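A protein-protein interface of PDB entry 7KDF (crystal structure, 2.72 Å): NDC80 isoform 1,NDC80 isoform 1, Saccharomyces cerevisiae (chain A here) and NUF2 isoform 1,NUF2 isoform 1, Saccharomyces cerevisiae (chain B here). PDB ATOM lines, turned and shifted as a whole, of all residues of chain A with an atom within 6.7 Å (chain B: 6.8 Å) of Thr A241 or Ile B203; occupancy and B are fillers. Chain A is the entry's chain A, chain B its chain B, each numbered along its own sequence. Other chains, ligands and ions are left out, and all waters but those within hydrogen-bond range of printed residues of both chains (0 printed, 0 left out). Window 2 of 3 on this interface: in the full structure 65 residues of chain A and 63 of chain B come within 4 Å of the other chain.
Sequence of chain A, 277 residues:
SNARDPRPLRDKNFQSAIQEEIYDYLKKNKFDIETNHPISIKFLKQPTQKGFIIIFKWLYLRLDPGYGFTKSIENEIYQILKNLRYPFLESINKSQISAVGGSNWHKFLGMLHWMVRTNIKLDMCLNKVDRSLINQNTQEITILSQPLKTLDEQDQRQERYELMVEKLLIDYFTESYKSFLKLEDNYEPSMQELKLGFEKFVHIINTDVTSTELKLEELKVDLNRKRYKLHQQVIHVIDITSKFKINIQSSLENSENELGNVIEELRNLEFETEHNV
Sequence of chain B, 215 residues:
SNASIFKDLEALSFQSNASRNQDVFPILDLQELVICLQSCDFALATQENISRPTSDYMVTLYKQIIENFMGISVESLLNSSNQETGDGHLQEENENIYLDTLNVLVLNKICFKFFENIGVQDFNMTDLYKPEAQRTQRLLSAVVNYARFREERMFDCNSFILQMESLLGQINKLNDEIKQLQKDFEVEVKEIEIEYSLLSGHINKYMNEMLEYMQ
His A236 touches none of the printed residues of chain B.
Thr A241 touches just one residue of chain B: Ile B203 (3.5 Å).
Ser B200 touches none of the printed residues of chain A.
Of the printed residues of chain A, Ile B203 touches Thr A241 (3.5 Å).
Of the printed residues of chain A, Tyr B206 touches Phe A244 and Lys A245.
Of the printed residues of chain A, Met B207 touches Phe A244.
The nearest residue of chain B that does not touch Thr A241 is Leu B199 (4.2 Å).
The nearest residue of chain A that does not touch Ile B203 is Phe A244 (4.5 Å).
Of the 11 printed residues of chain B, 4 touch a printed residue of chain A.
Along chain B the printed residues that touch a printed residue of chain A span positions 199 to 207.
Of the 11 printed residues of chain A, 4 touch a printed residue of chain B.
Printed residues of chain A that touch a printed residue of chain B: Val A237, Thr A241, Phe A244 and Lys A245.
Hydrophobic or aromatic side chains of chain A within 4 Å of the printed part of chain B: Val A237 and Phe A244.
Along chain A the printed residues that touch a printed residue of chain B span positions 237 to 245.
Among the printed residues, 5 pairs touch across the chains.
Among the printed residues, no Asp or Glu carboxylate lies within 4 Å of a Lys or Arg side-chain nitrogen of the other chain.
Among the printed residues, merely in contact across the chains: Thr A241 with Ile B203, Val A237 with Leu B199, Lys A245 with Tyr B206, Phe A244 with Tyr B206 and Phe A244 with Met B207.
The backbone carbonyl oxygen (O) of Val A237 sits at hydrogen-bond distance from the side-chain hydroxyl (OG1) of Thr A241.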
ATOM      1  N   HIS A 236      -1.049  21.158  -7.526  1.00  0.00           N
ATOM      2  CA  HIS A 236      -0.649  21.406  -6.146  1.00  0.00           C
ATOM      3  C   HIS A 236       0.721  20.807  -5.841  1.00  0.00           C
ATOM      4  O   HIS A 236       1.547  21.431  -5.165  1.00  0.00           O
ATOM      5  CB  HIS A 236      -1.707  20.835  -5.205  1.00  0.00           C
ATOM      6  CG  HIS A 236      -1.488  21.182  -3.766  1.00  0.00           C
ATOM      7  ND1 HIS A 236      -1.370  22.482  -3.321  1.00  0.00           N
ATOM      8  CD2 HIS A 236      -1.378  20.399  -2.668  1.00  0.00           C
ATOM      9  CE1 HIS A 236      -1.191  22.483  -2.012  1.00  0.00           C
ATOM     10  NE2 HIS A 236      -1.193  21.232  -1.591  1.00  0.00           N
ATOM     11  N   VAL A 237       0.969  19.586  -6.319  1.00  0.00           N
ATOM     12  CA  VAL A 237       2.258  18.939  -6.091  1.00  0.00           C
ATOM     13  C   VAL A 237       3.371  19.752  -6.735  1.00  0.00           C
ATOM     14  O   VAL A 237       4.397  20.044  -6.112  1.00  0.00           O
ATOM     15  CB  VAL A 237       2.233  17.499  -6.634  1.00  0.00           C
ATOM     16  CG1 VAL A 237       3.652  16.988  -6.859  1.00  0.00           C
ATOM     17  CG2 VAL A 237       1.453  16.588  -5.702  1.00  0.00           C
ATOM     18  N   ILE A 238       3.167  20.151  -7.989  1.00  0.00           N
ATOM     19  CA  ILE A 238       4.175  20.916  -8.709  1.00  0.00           C
ATOM     20  C   ILE A 238       4.340  22.302  -8.106  1.00  0.00           C
ATOM     21  O   ILE A 238       5.454  22.837  -8.043  1.00  0.00           O
ATOM     22  CB  ILE A 238       3.802  20.970 -10.196  1.00  0.00           C
ATOM     23  CG1 ILE A 238       3.694  19.536 -10.701  1.00  0.00           C
ATOM     24  CG2 ILE A 238       4.819  21.788 -10.979  1.00  0.00           C
ATOM     25  CD1 ILE A 238       3.515  19.397 -12.139  1.00  0.00           C
ATOM     26  N   ASP A 239       3.242  22.909  -7.652  1.00  0.00           N
ATOM     27  CA  ASP A 239       3.326  24.262  -7.112  1.00  0.00           C
ATOM     28  C   ASP A 239       4.194  24.314  -5.865  1.00  0.00           C
ATOM     29  O   ASP A 239       5.025  25.219  -5.721  1.00  0.00           O
ATOM     30  CB  ASP A 239       1.932  24.806  -6.804  1.00  0.00           C
ATOM     31  CG  ASP A 239       1.976  26.061  -5.951  1.00  0.00           C
ATOM     32  OD1 ASP A 239       2.379  27.123  -6.468  1.00  0.00           O
ATOM     33  OD2 ASP A 239       1.609  25.985  -4.761  1.00  0.00           O
ATOM     34  N   ILE A 240       4.029  23.361  -4.948  1.00  0.00           N
ATOM     35  CA  ILE A 240       4.752  23.471  -3.689  1.00  0.00           C
ATOM     36  C   ILE A 240       6.071  22.707  -3.706  1.00  0.00           C
ATOM     37  O   ILE A 240       6.953  23.010  -2.890  1.00  0.00           O
ATOM     38  CB  ILE A 240       3.911  23.016  -2.481  1.00  0.00           C
ATOM     39  CG1 ILE A 240       3.841  21.506  -2.412  1.00  0.00           C
ATOM     40  CG2 ILE A 240       2.487  23.569  -2.566  1.00  0.00           C
ATOM     41  CD1 ILE A 240       3.384  21.051  -1.075  1.00  0.00           C
ATOM     42  N   THR A 241       6.232  21.722  -4.595  1.00  0.00           N
ATOM     43  CA  THR A 241       7.551  21.121  -4.768  1.00  0.00           C
ATOM     44  C   THR A 241       8.539  22.153  -5.291  1.00  0.00           C
ATOM     45  O   THR A 241       9.654  22.284  -4.773  1.00  0.00           O
ATOM     46  CB  THR A 241       7.481  19.918  -5.713  1.00  0.00           C
ATOM     47  OG1 THR A 241       6.839  18.823  -5.051  1.00  0.00           O
ATOM     48  CG2 THR A 241       8.880  19.488  -6.140  1.00  0.00           C
ATOM     49  N   SER A 242       8.136  22.909  -6.313  1.00  0.00           N
ATOM     50  CA  SER A 242       9.004  23.953  -6.844  1.00  0.00           C
ATOM     51  C   SER A 242       9.240  25.050  -5.813  1.00  0.00           C
ATOM     52  O   SER A 242      10.372  25.522  -5.649  1.00  0.00           O
ATOM     53  CB  SER A 242       8.402  24.534  -8.122  1.00  0.00           C
ATOM     54  OG  SER A 242       7.161  25.157  -7.852  1.00  0.00           O
ATOM     55  N   LYS A 243       8.185  25.469  -5.109  1.00  0.00           N
ATOM     56  CA  LYS A 243       8.356  26.492  -4.080  1.00  0.00           C
ATOM     57  C   LYS A 243       9.271  25.994  -2.969  1.00  0.00           C
ATOM     58  O   LYS A 243      10.092  26.752  -2.443  1.00  0.00           O
ATOM     59  CB  LYS A 243       6.997  26.917  -3.514  1.00  0.00           C
ATOM     60  CG  LYS A 243       7.113  27.986  -2.435  1.00  0.00           C
ATOM     61  CD  LYS A 243       5.779  28.604  -2.044  1.00  0.00           C
ATOM     62  CE  LYS A 243       5.996  29.726  -1.025  1.00  0.00           C
ATOM     63  NZ  LYS A 243       4.744  30.454  -0.667  1.00  0.00           N
ATOM     64  N   PHE A 244       9.141  24.717  -2.607  1.00  0.00           N
ATOM     65  CA  PHE A 244      10.034  24.105  -1.630  1.00  0.00           C
ATOM     66  C   PHE A 244      11.492  24.217  -2.067  1.00  0.00           C
ATOM     67  O   PHE A 244      12.340  24.721  -1.319  1.00  0.00           O
ATOM     68  CB  PHE A 244       9.612  22.647  -1.441  1.00  0.00           C
ATOM     69  CG  PHE A 244      10.560  21.808  -0.641  1.00  0.00           C
ATOM     70  CD1 PHE A 244      10.602  21.899   0.740  1.00  0.00           C
ATOM     71  CD2 PHE A 244      11.366  20.875  -1.273  1.00  0.00           C
ATOM     72  CE1 PHE A 244      11.457  21.097   1.472  1.00  0.00           C
ATOM     73  CE2 PHE A 244      12.224  20.072  -0.550  1.00  0.00           C
ATOM     74  CZ  PHE A 244      12.272  20.183   0.825  1.00  0.00           C
ATOM     75  N   LYS A 245      11.796  23.784  -3.294  1.00  0.00           N
ATOM     76  CA  LYS A 245      13.185  23.720  -3.738  1.00  0.00           C
ATOM     77  C   LYS A 245      13.798  25.106  -3.855  1.00  0.00           C
ATOM     78  O   LYS A 245      14.938  25.329  -3.420  1.00  0.00           O
ATOM     79  CB  LYS A 245      13.276  22.977  -5.070  1.00  0.00           C
ATOM     80  CG  LYS A 245      14.699  22.619  -5.462  1.00  0.00           C
ATOM     81  CD  LYS A 245      15.433  21.964  -4.303  1.00  0.00           C
ATOM     82  CE  LYS A 245      16.531  21.036  -4.794  1.00  0.00           C
ATOM     83  NZ  LYS A 245      17.497  21.729  -5.687  1.00  0.00           N
ATOM     84  N   ILE A 246      13.051  26.053  -4.426  1.00  0.00           N
ATOM     85  CA  ILE A 246      13.569  27.407  -4.588  1.00  0.00           C
ATOM     86  C   ILE A 246      13.784  28.070  -3.234  1.00  0.00           C
ATOM     87  O   ILE A 246      14.738  28.836  -3.047  1.00  0.00           O
ATOM     88  CB  ILE A 246      12.646  28.236  -5.505  1.00  0.00           C
ATOM     89  CG1 ILE A 246      12.658  27.622  -6.908  1.00  0.00           C
ATOM     90  CG2 ILE A 246      13.003  29.721  -5.491  1.00  0.00           C
ATOM     91  CD1 ILE A 246      11.664  28.215  -7.885  1.00  0.00           C
ATOM     92  N   LEU B 198       7.903   8.464  -8.623  1.00  0.00           N
ATOM     93  CA  LEU B 198       9.288   8.842  -8.881  1.00  0.00           C
ATOM     94  C   LEU B 198       9.631  10.150  -8.179  1.00  0.00           C
ATOM     95  O   LEU B 198      10.667  10.261  -7.512  1.00  0.00           O
ATOM     96  CB  LEU B 198       9.524   8.964 -10.386  1.00  0.00           C
ATOM     97  CG  LEU B 198       9.450   7.656 -11.174  1.00  0.00           C
ATOM     98  CD1 LEU B 198       9.762   7.880 -12.651  1.00  0.00           C
ATOM     99  CD2 LEU B 198      10.395   6.627 -10.563  1.00  0.00           C
ATOM    100  N   LEU B 199       8.756  11.148  -8.304  1.00  0.00           N
ATOM    101  CA  LEU B 199       9.011  12.437  -7.672  1.00  0.00           C
ATOM    102  C   LEU B 199       8.983  12.324  -6.153  1.00  0.00           C
ATOM    103  O   LEU B 199       9.769  12.982  -5.464  1.00  0.00           O
ATOM    104  CB  LEU B 199       7.994  13.467  -8.162  1.00  0.00           C
ATOM    105  CG  LEU B 199       8.016  14.816  -7.447  1.00  0.00           C
ATOM    106  CD1 LEU B 199       9.299  15.547  -7.778  1.00  0.00           C
ATOM    107  CD2 LEU B 199       6.821  15.640  -7.865  1.00  0.00           C
ATOM    108  N   SER B 200       8.081  11.501  -5.611  1.00  0.00           N
ATOM    109  CA  SER B 200       8.028  11.317  -4.164  1.00  0.00           C
ATOM    110  C   SER B 200       9.316  10.695  -3.642  1.00  0.00           C
ATOM    111  O   SER B 200       9.844  11.119  -2.607  1.00  0.00           O
ATOM    112  CB  SER B 200       6.828  10.453  -3.780  1.00  0.00           C
ATOM    113  OG  SER B 200       6.810  10.213  -2.383  1.00  0.00           O
ATOM    114  N   GLY B 201       9.832   9.686  -4.343  1.00  0.00           N
ATOM    115  CA  GLY B 201      11.108   9.109  -3.955  1.00  0.00           C
ATOM    116  C   GLY B 201      12.251  10.091  -4.106  1.00  0.00           C
ATOM    117  O   GLY B 201      13.181  10.105  -3.293  1.00  0.00           O
ATOM    118  N   HIS B 202      12.194  10.929  -5.144  1.00  0.00           N
ATOM    119  CA  HIS B 202      13.229  11.934  -5.364  1.00  0.00           C
ATOM    120  C   HIS B 202      13.294  12.934  -4.214  1.00  0.00           C
ATOM    121  O   HIS B 202      14.385  13.295  -3.759  1.00  0.00           O
ATOM    122  CB  HIS B 202      12.971  12.651  -6.690  1.00  0.00           C
ATOM    123  CG  HIS B 202      14.155  13.390  -7.227  1.00  0.00           C
ATOM    124  ND1 HIS B 202      15.129  12.783  -7.991  1.00  0.00           N
ATOM    125  CD2 HIS B 202      14.510  14.693  -7.132  1.00  0.00           C
ATOM    126  CE1 HIS B 202      16.038  13.678  -8.332  1.00  0.00           C
ATOM    127  NE2 HIS B 202      15.685  14.846  -7.825  1.00  0.00           N
ATOM    128  N   ILE B 203      12.137  13.398  -3.734  1.00  0.00           N
ATOM    129  CA  ILE B 203      12.118  14.368  -2.643  1.00  0.00           C
ATOM    130  C   ILE B 203      12.588  13.731  -1.339  1.00  0.00           C
ATOM    131  O   ILE B 203      13.337  14.348  -0.570  1.00  0.00           O
ATOM    132  CB  ILE B 203      10.712  14.980  -2.507  1.00  0.00           C
ATOM    133  CG1 ILE B 203      10.320  15.711  -3.794  1.00  0.00           C
ATOM    134  CG2 ILE B 203      10.638  15.914  -1.305  1.00  0.00           C
ATOM    135  CD1 ILE B 203       8.942  16.336  -3.750  1.00  0.00           C
ATOM    136  N   ASN B 204      12.138  12.499  -1.058  1.00  0.00           N
ATOM    137  CA  ASN B 204      12.638  11.767   0.105  1.00  0.00           C
ATOM    138  C   ASN B 204      14.126  11.478   0.004  1.00  0.00           C
ATOM    139  O   ASN B 204      14.845  11.584   1.003  1.00  0.00           O
ATOM    140  CB  ASN B 204      11.841  10.478   0.308  1.00  0.00           C
ATOM    141  CG  ASN B 204      10.494  10.721   0.961  1.00  0.00           C
ATOM    142  OD1 ASN B 204       9.441  10.626   0.332  1.00  0.00           O
ATOM    143  ND2 ASN B 204      10.527  10.902   2.283  1.00  0.00           N
ATOM    144  N   LYS B 205      14.608  11.093  -1.178  1.00  0.00           N
ATOM    145  CA  LYS B 205      16.044  10.904  -1.347  1.00  0.00           C
ATOM    146  C   LYS B 205      16.792  12.201  -1.041  1.00  0.00           C
ATOM    147  O   LYS B 205      17.765  12.204  -0.277  1.00  0.00           O
ATOM    148  CB  LYS B 205      16.335  10.405  -2.763  1.00  0.00           C
ATOM    149  CG  LYS B 205      17.803  10.113  -3.058  1.00  0.00           C
ATOM    150  CD  LYS B 205      17.940   9.599  -4.485  1.00  0.00           C
ATOM    151  CE  LYS B 205      19.403   9.389  -4.863  1.00  0.00           C
ATOM    152  NZ  LYS B 205      19.444   8.894  -6.273  1.00  0.00           N
ATOM    153  N   TYR B 206      16.299  13.321  -1.580  1.00  0.00           N
ATOM    154  CA  TYR B 206      16.894  14.639  -1.349  1.00  0.00           C
ATOM    155  C   TYR B 206      17.002  14.977   0.139  1.00  0.00           C
ATOM    156  O   TYR B 206      18.059  15.403   0.617  1.00  0.00           O
ATOM    157  CB  TYR B 206      16.052  15.685  -2.079  1.00  0.00           C
ATOM    158  CG  TYR B 206      16.406  17.123  -1.806  1.00  0.00           C
ATOM    159  CD1 TYR B 206      17.563  17.682  -2.329  1.00  0.00           C
ATOM    160  CD2 TYR B 206      15.569  17.931  -1.050  1.00  0.00           C
ATOM    161  CE1 TYR B 206      17.887  19.000  -2.096  1.00  0.00           C
ATOM    162  CE2 TYR B 206      15.885  19.252  -0.810  1.00  0.00           C
ATOM    163  CZ  TYR B 206      17.047  19.782  -1.334  1.00  0.00           C
ATOM    164  OH  TYR B 206      17.370  21.098  -1.096  1.00  0.00           O
ATOM    165  N   MET B 207      15.912  14.804   0.886  1.00  0.00           N
ATOM    166  CA  MET B 207      15.945  15.119   2.310  1.00  0.00           C
ATOM    167  C   MET B 207      16.923  14.215   3.051  1.00  0.00           C
ATOM    168  O   MET B 207      17.632  14.666   3.955  1.00  0.00           O
ATOM    169  CB  MET B 207      14.545  14.993   2.902  1.00  0.00           C
ATOM    170  CG  MET B 207      13.608  16.078   2.452  1.00  0.00           C
ATOM    171  SD  MET B 207      11.904  15.593   2.756  1.00  0.00           S
ATOM    172  CE  MET B 207      11.225  17.158   3.217  1.00  0.00           C
ATOM    173  N   ASN B 208      16.979  12.936   2.674  1.00  0.00           N
ATOM    174  CA  ASN B 208      17.855  12.005   3.378  1.00  0.00           C
ATOM    175  C   ASN B 208      19.319  12.407   3.238  1.00  0.00           C
ATOM    176  O   ASN B 208      20.075  12.370   4.216  1.00  0.00           O
ATOM    177  CB  ASN B 208      17.630  10.583   2.866  1.00  0.00           C
ATOM    178  CG  ASN B 208      16.237  10.064   3.175  1.00  0.00           C
ATOM    179  OD1 ASN B 208      15.604  10.486   4.147  1.00  0.00           O
ATOM    180  ND2 ASN B 208      15.748   9.146   2.345  1.00  0.00           N
